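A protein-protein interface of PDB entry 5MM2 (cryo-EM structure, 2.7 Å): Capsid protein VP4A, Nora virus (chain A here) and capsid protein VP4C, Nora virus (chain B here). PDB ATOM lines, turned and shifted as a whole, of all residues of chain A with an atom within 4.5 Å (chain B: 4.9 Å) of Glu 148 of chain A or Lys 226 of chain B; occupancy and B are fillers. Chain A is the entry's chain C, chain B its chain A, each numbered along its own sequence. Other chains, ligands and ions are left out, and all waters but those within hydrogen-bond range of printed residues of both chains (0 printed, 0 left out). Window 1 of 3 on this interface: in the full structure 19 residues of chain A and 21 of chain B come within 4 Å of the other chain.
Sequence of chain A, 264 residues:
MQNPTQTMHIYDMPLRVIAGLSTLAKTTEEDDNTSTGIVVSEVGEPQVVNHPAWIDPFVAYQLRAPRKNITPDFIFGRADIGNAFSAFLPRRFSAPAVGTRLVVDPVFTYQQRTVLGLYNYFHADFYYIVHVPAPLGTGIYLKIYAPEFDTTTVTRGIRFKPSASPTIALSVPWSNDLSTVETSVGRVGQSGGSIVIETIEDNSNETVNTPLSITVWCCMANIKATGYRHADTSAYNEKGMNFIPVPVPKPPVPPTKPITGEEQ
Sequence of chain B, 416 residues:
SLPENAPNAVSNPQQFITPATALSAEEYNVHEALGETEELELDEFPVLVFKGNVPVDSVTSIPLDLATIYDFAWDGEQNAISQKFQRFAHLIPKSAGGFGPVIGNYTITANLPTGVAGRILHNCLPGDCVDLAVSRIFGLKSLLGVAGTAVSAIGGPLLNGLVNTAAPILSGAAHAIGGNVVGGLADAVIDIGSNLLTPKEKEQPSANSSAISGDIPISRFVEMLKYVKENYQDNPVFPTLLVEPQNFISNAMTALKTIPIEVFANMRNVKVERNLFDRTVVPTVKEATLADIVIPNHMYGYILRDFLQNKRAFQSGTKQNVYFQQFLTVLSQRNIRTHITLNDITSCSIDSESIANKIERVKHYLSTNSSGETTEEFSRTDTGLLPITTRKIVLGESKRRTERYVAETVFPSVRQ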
ATOM      1  N   ALA A 146     -28.910 -13.988  11.862  1.00  0.00           N
ATOM      2  CA  ALA A 146     -27.608 -13.337  11.972  1.00  0.00           C
ATOM      3  C   ALA A 146     -26.824 -13.881  13.154  1.00  0.00           C
ATOM      4  O   ALA A 146     -27.366 -13.944  14.263  1.00  0.00           O
ATOM      5  CB  ALA A 146     -27.777 -11.831  12.122  1.00  0.00           C
ATOM      6  N   PRO A 147     -25.559 -14.248  12.976  1.00  0.00           N
ATOM      7  CA  PRO A 147     -24.802 -14.877  14.061  1.00  0.00           C
ATOM      8  C   PRO A 147     -24.346 -13.850  15.075  1.00  0.00           C
ATOM      9  O   PRO A 147     -24.199 -12.668  14.765  1.00  0.00           O
ATOM     10  CB  PRO A 147     -23.604 -15.487  13.330  1.00  0.00           C
ATOM     11  CG  PRO A 147     -23.400 -14.580  12.192  1.00  0.00           C
ATOM     12  CD  PRO A 147     -24.738 -14.078  11.771  1.00  0.00           C
ATOM     13  N   GLU A 148     -24.137 -14.298  16.314  1.00  0.00           N
ATOM     14  CA  GLU A 148     -23.818 -13.331  17.355  1.00  0.00           C
ATOM     15  C   GLU A 148     -22.461 -13.536  18.014  1.00  0.00           C
ATOM     16  O   GLU A 148     -21.603 -12.656  17.900  1.00  0.00           O
ATOM     17  CB  GLU A 148     -24.930 -13.327  18.403  1.00  0.00           C
ATOM     18  CG  GLU A 148     -24.758 -12.212  19.391  1.00  0.00           C
ATOM     19  CD  GLU A 148     -24.889 -10.838  18.761  1.00  0.00           C
ATOM     20  OE1 GLU A 148     -25.635 -10.675  17.774  1.00  0.00           O
ATOM     21  OE2 GLU A 148     -24.217  -9.910  19.246  1.00  0.00           O
ATOM     22  N   PHE A 149     -22.218 -14.657  18.693  1.00  0.00           N
ATOM     23  CA  PHE A 149     -20.964 -14.838  19.422  1.00  0.00           C
ATOM     24  C   PHE A 149     -20.157 -16.019  18.914  1.00  0.00           C
ATOM     25  O   PHE A 149     -18.959 -15.875  18.660  1.00  0.00           O
ATOM     26  CB  PHE A 149     -21.194 -15.007  20.930  1.00  0.00           C
ATOM     27  CG  PHE A 149     -21.509 -13.739  21.654  1.00  0.00           C
ATOM     28  CD1 PHE A 149     -20.515 -12.827  21.927  1.00  0.00           C
ATOM     29  CD2 PHE A 149     -22.778 -13.488  22.118  1.00  0.00           C
ATOM     30  CE1 PHE A 149     -20.791 -11.666  22.608  1.00  0.00           C
ATOM     31  CE2 PHE A 149     -23.056 -12.328  22.811  1.00  0.00           C
ATOM     32  CZ  PHE A 149     -22.062 -11.423  23.055  1.00  0.00           C
ATOM     33  N   ASP A 150     -20.765 -17.183  18.778  1.00  0.00           N
ATOM     34  CA  ASP A 150     -20.045 -18.406  18.480  1.00  0.00           C
ATOM     35  C   ASP A 150     -20.831 -19.259  17.492  1.00  0.00           C
ATOM     36  O   ASP A 150     -21.726 -18.783  16.802  1.00  0.00           O
ATOM     37  CB  ASP A 150     -19.730 -19.141  19.781  1.00  0.00           C
ATOM     38  CG  ASP A 150     -20.955 -19.388  20.626  1.00  0.00           C
ATOM     39  OD1 ASP A 150     -22.064 -18.966  20.252  1.00  0.00           O
ATOM     40  OD2 ASP A 150     -20.803 -19.977  21.706  1.00  0.00           O
ATOM     41  N   THR A 153     -24.996 -20.284  18.543  1.00  0.00           N
ATOM     42  CA  THR A 153     -25.972 -19.331  19.054  1.00  0.00           C
ATOM     43  C   THR A 153     -26.985 -18.962  17.977  1.00  0.00           C
ATOM     44  O   THR A 153     -26.608 -18.603  16.861  1.00  0.00           O
ATOM     45  CB  THR A 153     -25.252 -18.090  19.562  1.00  0.00           C
ATOM     46  OG1 THR A 153     -24.304 -18.476  20.559  1.00  0.00           O
ATOM     47  CG2 THR A 153     -26.222 -17.126  20.172  1.00  0.00           C
ATOM     48  N   THR A 155     -30.475 -16.712  16.905  1.00  0.00           N
ATOM     49  CA  THR A 155     -31.265 -15.527  17.206  1.00  0.00           C
ATOM     50  C   THR A 155     -32.584 -15.571  16.436  1.00  0.00           C
ATOM     51  O   THR A 155     -32.899 -16.541  15.752  1.00  0.00           O
ATOM     52  CB  THR A 155     -30.499 -14.247  16.870  1.00  0.00           C
ATOM     53  OG1 THR A 155     -30.281 -14.186  15.463  1.00  0.00           O
ATOM     54  CG2 THR A 155     -29.161 -14.227  17.557  1.00  0.00           C
ATOM     55  N   ASP A 177     -20.404  -2.934  19.526  1.00  0.00           N
ATOM     56  CA  ASP A 177     -20.189  -2.129  20.724  1.00  0.00           C
ATOM     57  C   ASP A 177     -19.131  -1.061  20.530  1.00  0.00           C
ATOM     58  O   ASP A 177     -18.971  -0.195  21.391  1.00  0.00           O
ATOM     59  CB  ASP A 177     -19.822  -3.007  21.917  1.00  0.00           C
ATOM     60  CG  ASP A 177     -18.599  -3.843  21.682  1.00  0.00           C
ATOM     61  OD1 ASP A 177     -18.123  -3.927  20.539  1.00  0.00           O
ATOM     62  OD2 ASP A 177     -18.087  -4.413  22.667  1.00  0.00           O
ATOM     63  N   GLY A 189     -15.304 -10.989  18.328  1.00  0.00           N
ATOM     64  CA  GLY A 189     -16.660 -11.231  18.749  1.00  0.00           C
ATOM     65  C   GLY A 189     -17.698 -10.391  18.052  1.00  0.00           C
ATOM     66  O   GLY A 189     -18.853 -10.381  18.483  1.00  0.00           O
ATOM     67  N   GLN A 190     -17.330  -9.694  16.988  1.00  0.00           N
ATOM     68  CA  GLN A 190     -18.272  -8.835  16.303  1.00  0.00           C
ATOM     69  C   GLN A 190     -19.178  -9.645  15.390  1.00  0.00           C
ATOM     70  O   GLN A 190     -18.885 -10.782  15.025  1.00  0.00           O
ATOM     71  CB  GLN A 190     -17.546  -7.782  15.478  1.00  0.00           C
ATOM     72  CG  GLN A 190     -16.792  -8.341  14.302  1.00  0.00           C
ATOM     73  CD  GLN A 190     -16.152  -7.266  13.483  1.00  0.00           C
ATOM     74  OE1 GLN A 190     -16.270  -6.089  13.793  1.00  0.00           O
ATOM     75  NE2 GLN A 190     -15.503  -7.653  12.408  1.00  0.00           N
ATOM     76  N   SER A 191     -20.301  -9.038  15.025  1.00  0.00           N
ATOM     77  CA  SER A 191     -21.206  -9.635  14.057  1.00  0.00           C
ATOM     78  C   SER A 191     -20.811  -9.280  12.633  1.00  0.00           C
ATOM     79  O   SER A 191     -20.727 -10.160  11.776  1.00  0.00           O
ATOM     80  CB  SER A 191     -22.637  -9.181  14.328  1.00  0.00           C
ATOM     81  OG  SER A 191     -23.061  -9.631  15.593  1.00  0.00           O
ATOM     82  N   ALA B  89     -27.343 -10.203  24.505  1.00  0.00           N
ATOM     83  CA  ALA B  89     -26.013  -9.836  24.053  1.00  0.00           C
ATOM     84  C   ALA B  89     -25.666  -8.409  24.417  1.00  0.00           C
ATOM     85  O   ALA B  89     -24.536  -8.125  24.813  1.00  0.00           O
ATOM     86  CB  ALA B  89     -25.897 -10.011  22.543  1.00  0.00           C
ATOM     87  N   HIS B  90     -26.625  -7.507  24.297  1.00  0.00           N
ATOM     88  CA  HIS B  90     -26.384  -6.080  24.399  1.00  0.00           C
ATOM     89  C   HIS B  90     -27.115  -5.551  25.614  1.00  0.00           C
ATOM     90  O   HIS B  90     -28.315  -5.779  25.764  1.00  0.00           O
ATOM     91  CB  HIS B  90     -26.898  -5.364  23.161  1.00  0.00           C
ATOM     92  CG  HIS B  90     -26.277  -5.837  21.892  1.00  0.00           C
ATOM     93  ND1 HIS B  90     -26.814  -5.544  20.660  1.00  0.00           N
ATOM     94  CD2 HIS B  90     -25.157  -6.554  21.656  1.00  0.00           C
ATOM     95  CE1 HIS B  90     -26.061  -6.081  19.719  1.00  0.00           C
ATOM     96  NE2 HIS B  90     -25.053  -6.703  20.298  1.00  0.00           N
ATOM     97  N   MET B 224     -22.352   0.014  23.750  1.00  0.00           N
ATOM     98  CA  MET B 224     -23.255  -0.843  24.498  1.00  0.00           C
ATOM     99  C   MET B 224     -22.374  -1.726  25.368  1.00  0.00           C
ATOM    100  O   MET B 224     -21.186  -1.447  25.543  1.00  0.00           O
ATOM    101  CB  MET B 224     -24.158  -1.621  23.531  1.00  0.00           C
ATOM    102  CG  MET B 224     -23.360  -2.486  22.608  1.00  0.00           C
ATOM    103  SD  MET B 224     -24.247  -3.195  21.236  1.00  0.00           S
ATOM    104  CE  MET B 224     -24.483  -1.755  20.212  1.00  0.00           C
ATOM    105  N   LEU B 225     -22.926  -2.803  25.902  1.00  0.00           N
ATOM    106  CA  LEU B 225     -22.197  -3.576  26.892  1.00  0.00           C
ATOM    107  C   LEU B 225     -22.143  -5.039  26.475  1.00  0.00           C
ATOM    108  O   LEU B 225     -22.627  -5.934  27.164  1.00  0.00           O
ATOM    109  CB  LEU B 225     -22.823  -3.351  28.258  1.00  0.00           C
ATOM    110  CG  LEU B 225     -21.969  -3.359  29.514  1.00  0.00           C
ATOM    111  CD1 LEU B 225     -22.694  -2.553  30.554  1.00  0.00           C
ATOM    112  CD2 LEU B 225     -21.718  -4.731  30.023  1.00  0.00           C
ATOM    113  N   LYS B 226     -21.637  -5.288  25.272  1.00  0.00           N
ATOM    114  CA  LYS B 226     -21.396  -6.650  24.808  1.00  0.00           C
ATOM    115  C   LYS B 226     -20.166  -7.240  25.482  1.00  0.00           C
ATOM    116  O   LYS B 226     -19.057  -6.730  25.312  1.00  0.00           O
ATOM    117  CB  LYS B 226     -21.218  -6.657  23.298  1.00  0.00           C
ATOM    118  CG  LYS B 226     -20.927  -8.023  22.759  1.00  0.00           C
ATOM    119  CD  LYS B 226     -20.668  -8.012  21.279  1.00  0.00           C
ATOM    120  CE  LYS B 226     -21.936  -7.850  20.504  1.00  0.00           C
ATOM    121  NZ  LYS B 226     -21.696  -8.003  19.052  1.00  0.00           N
ATOM    122  N   TYR B 227     -20.347  -8.329  26.214  1.00  0.00           N
ATOM    123  CA  TYR B 227     -19.293  -8.942  27.011  1.00  0.00           C
ATOM    124  C   TYR B 227     -18.636 -10.080  26.240  1.00  0.00           C
ATOM    125  O   TYR B 227     -19.325 -10.980  25.756  1.00  0.00           O
ATOM    126  CB  TYR B 227     -19.878  -9.462  28.320  1.00  0.00           C
ATOM    127  CG  TYR B 227     -18.885 -10.121  29.232  1.00  0.00           C
ATOM    128  CD1 TYR B 227     -18.050  -9.373  30.039  1.00  0.00           C
ATOM    129  CD2 TYR B 227     -18.786 -11.497  29.289  1.00  0.00           C
ATOM    130  CE1 TYR B 227     -17.146  -9.975  30.867  1.00  0.00           C
ATOM    131  CE2 TYR B 227     -17.887 -12.103  30.104  1.00  0.00           C
ATOM    132  CZ  TYR B 227     -17.072 -11.339  30.897  1.00  0.00           C
ATOM    133  OH  TYR B 227     -16.171 -11.949  31.724  1.00  0.00           O
ATOM    134  N   VAL B 228     -17.305 -10.054  26.141  1.00  0.00           N
ATOM    135  CA  VAL B 228     -16.584 -11.076  25.385  1.00  0.00           C
ATOM    136  C   VAL B 228     -15.596 -11.831  26.276  1.00  0.00           C
ATOM    137  O   VAL B 228     -15.367 -13.031  26.067  1.00  0.00           O
ATOM    138  CB  VAL B 228     -15.900 -10.441  24.157  1.00  0.00           C
ATOM    139  CG1 VAL B 228     -15.072 -11.433  23.380  1.00  0.00           C
ATOM    140  CG2 VAL B 228     -16.936  -9.867  23.225  1.00  0.00           C
ATOM    141  N   TYR B 232     -12.368  -7.455  27.348  1.00  0.00           N
ATOM    142  CA  TYR B 232     -12.411  -6.670  28.569  1.00  0.00           C
ATOM    143  C   TYR B 232     -11.194  -6.897  29.442  1.00  0.00           C
ATOM    144  O   TYR B 232     -11.026  -6.194  30.436  1.00  0.00           O
ATOM    145  CB  TYR B 232     -13.675  -6.951  29.383  1.00  0.00           C
ATOM    146  CG  TYR B 232     -14.963  -6.425  28.790  1.00  0.00           C
ATOM    147  CD1 TYR B 232     -14.979  -5.721  27.600  1.00  0.00           C
ATOM    148  CD2 TYR B 232     -16.147  -6.539  29.485  1.00  0.00           C
ATOM    149  CE1 TYR B 232     -16.147  -5.242  27.077  1.00  0.00           C
ATOM    150  CE2 TYR B 232     -17.318  -6.044  28.977  1.00  0.00           C
ATOM    151  CZ  TYR B 232     -17.308  -5.389  27.780  1.00  0.00           C
ATOM    152  OH  TYR B 232     -18.481  -4.895  27.273  1.00  0.00           O
ATOM    153  N   ARG B 274     -31.096  -8.111  21.483  1.00  0.00           N
ATOM    154  CA  ARG B 274     -30.452  -9.288  20.891  1.00  0.00           C
ATOM    155  C   ARG B 274     -30.477 -10.478  21.856  1.00  0.00           C
ATOM    156  O   ARG B 274     -29.485 -10.887  22.449  1.00  0.00           O
ATOM    157  CB  ARG B 274     -29.047  -8.899  20.407  1.00  0.00           C
ATOM    158  CG  ARG B 274     -28.229  -9.907  19.639  1.00  0.00           C
ATOM    159  CD  ARG B 274     -28.971 -10.429  18.444  1.00  0.00           C
ATOM    160  NE  ARG B 274     -29.591  -9.367  17.669  1.00  0.00           N
ATOM    161  CZ  ARG B 274     -30.491  -9.601  16.730  1.00  0.00           C
ATOM    162  NH1 ARG B 274     -30.825 -10.844  16.439  1.00  0.00           N
ATOM    163  NH2 ARG B 274     -31.057  -8.606  16.092  1.00  0.00           N
ATOM    164  N   LEU B 276     -30.635 -14.153  23.053  1.00  0.00           N
ATOM    165  CA  LEU B 276     -29.806 -15.238  22.539  1.00  0.00           C
ATOM    166  C   LEU B 276     -30.291 -16.601  23.010  1.00  0.00           C
ATOM    167  O   LEU B 276     -30.684 -16.766  24.164  1.00  0.00           O
ATOM    168  CB  LEU B 276     -28.363 -15.062  22.978  1.00  0.00           C
ATOM    169  CG  LEU B 276     -27.747 -13.761  22.508  1.00  0.00           C
ATOM    170  CD1 LEU B 276     -26.371 -13.670  23.042  1.00  0.00           C
ATOM    171  CD2 LEU B 276     -27.735 -13.702  21.015  1.00  0.00           C
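A ring nitrogen (NE2) of His 90 of chain B sits at hydrogen-bond distance from the side-chain carboxylate of Glu 148 of chain A (3.5 Å). The side-chain carboxylate (OE2) of Glu 148 of chain A is in salt-bridge range of the side-chain amino group (NZ) of Lys 226 of chain B (3.2 Å).
The backbone NH (N) of Ala 89 of chain B is in hydrogen-bond range of the backbone carbonyl oxygen (O) of Arg 274 of chain B (3.0 Å). The side-chain hydroxyl (OH) of Tyr 232 of chain B lies within hydrogen-bond range of the backbone carbonyl oxygen (O) of Lys 226 of chain B (2.7 Å). O of Ala 146 of chain A sits at hydrogen-bond distance from OG1 of Thr 155 of chain A, 3.2 Å away. The side-chain sulfur (SD) of Met 224 of chain B lies close to a ring nitrogen (ND1) of His 90 of chain B (3.5 Å).
Among the printed residues, merely in contact across the chains: Glu 148 of chain A with Arg 274 of chain B (3.3 Å), Thr 155 of chain A with Arg 274 of chain B (3.4 Å), Phe 149 of chain A with Tyr 227 of chain B (3.5 Å), Phe 149 of chain A with Leu 276 of chain B (3.6 Å), Phe 149 of chain A with Lys 226 of chain B (3.6 Å), Asp 177 of chain A with Met 224 of chain B (3.6 Å), Asp 177 of chain A with Lys 226 of chain B (3.6 Å), Phe 149 of chain A with Ala 89 of chain B (3.7 Å), Glu 148 of chain A with Ala 89 of chain B (3.7 Å), Glu 148 of chain A with Leu 276 of chain B (3.7 Å), Gly 189 of chain A with Lys 226 of chain B (3.7 Å), Thr 155 of chain A with Leu 276 of chain B (3.8 Å) and Thr 153 of chain A with Leu 276 of chain B (3.8 Å).
Glu 148 of chain A touches just these residues of chain B: Ala 89, His 90, Lys 226, Arg 274 and Leu 276. Lys 226 of chain B touches just these residues of chain A: Glu 148, Phe 149, Asp 177 and Gly 189. Of the printed residues of chain A, Arg 274 of chain B touches Glu 148 (3.3 Å) and Thr 155 (3.4 Å). Of the printed residues of chain A, Ala 89 of chain B touches Glu 148 and Phe 149. Of the printed residues of chain A, His 90 of chain B touches Glu 148. Of the printed residues of chain A, Tyr 227 of chain B touches Phe 149 (3.5 Å). Printed residues of chain A within 4 Å of Met 224 of chain B: Asp 177. Pro 147 of chain A touches none of the printed residues of chain B. Tyr 232 of chain B touches none of the printed residues of chain A. The nearest printed residue of chain B that does not touch Glu 148 of chain A is Met 224 of chain B (7.0 Å). The nearest residue of chain A that does not touch Lys 226 of chain B is Ser 191 of chain A (4.1 Å).
Of the 10 printed residues of chain B, 7 touch a printed residue of chain A. Hydrophobic or aromatic side chains of chain B that line the printed part of chain A: Ala 89, His 90, Met 224 and Leu 276.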
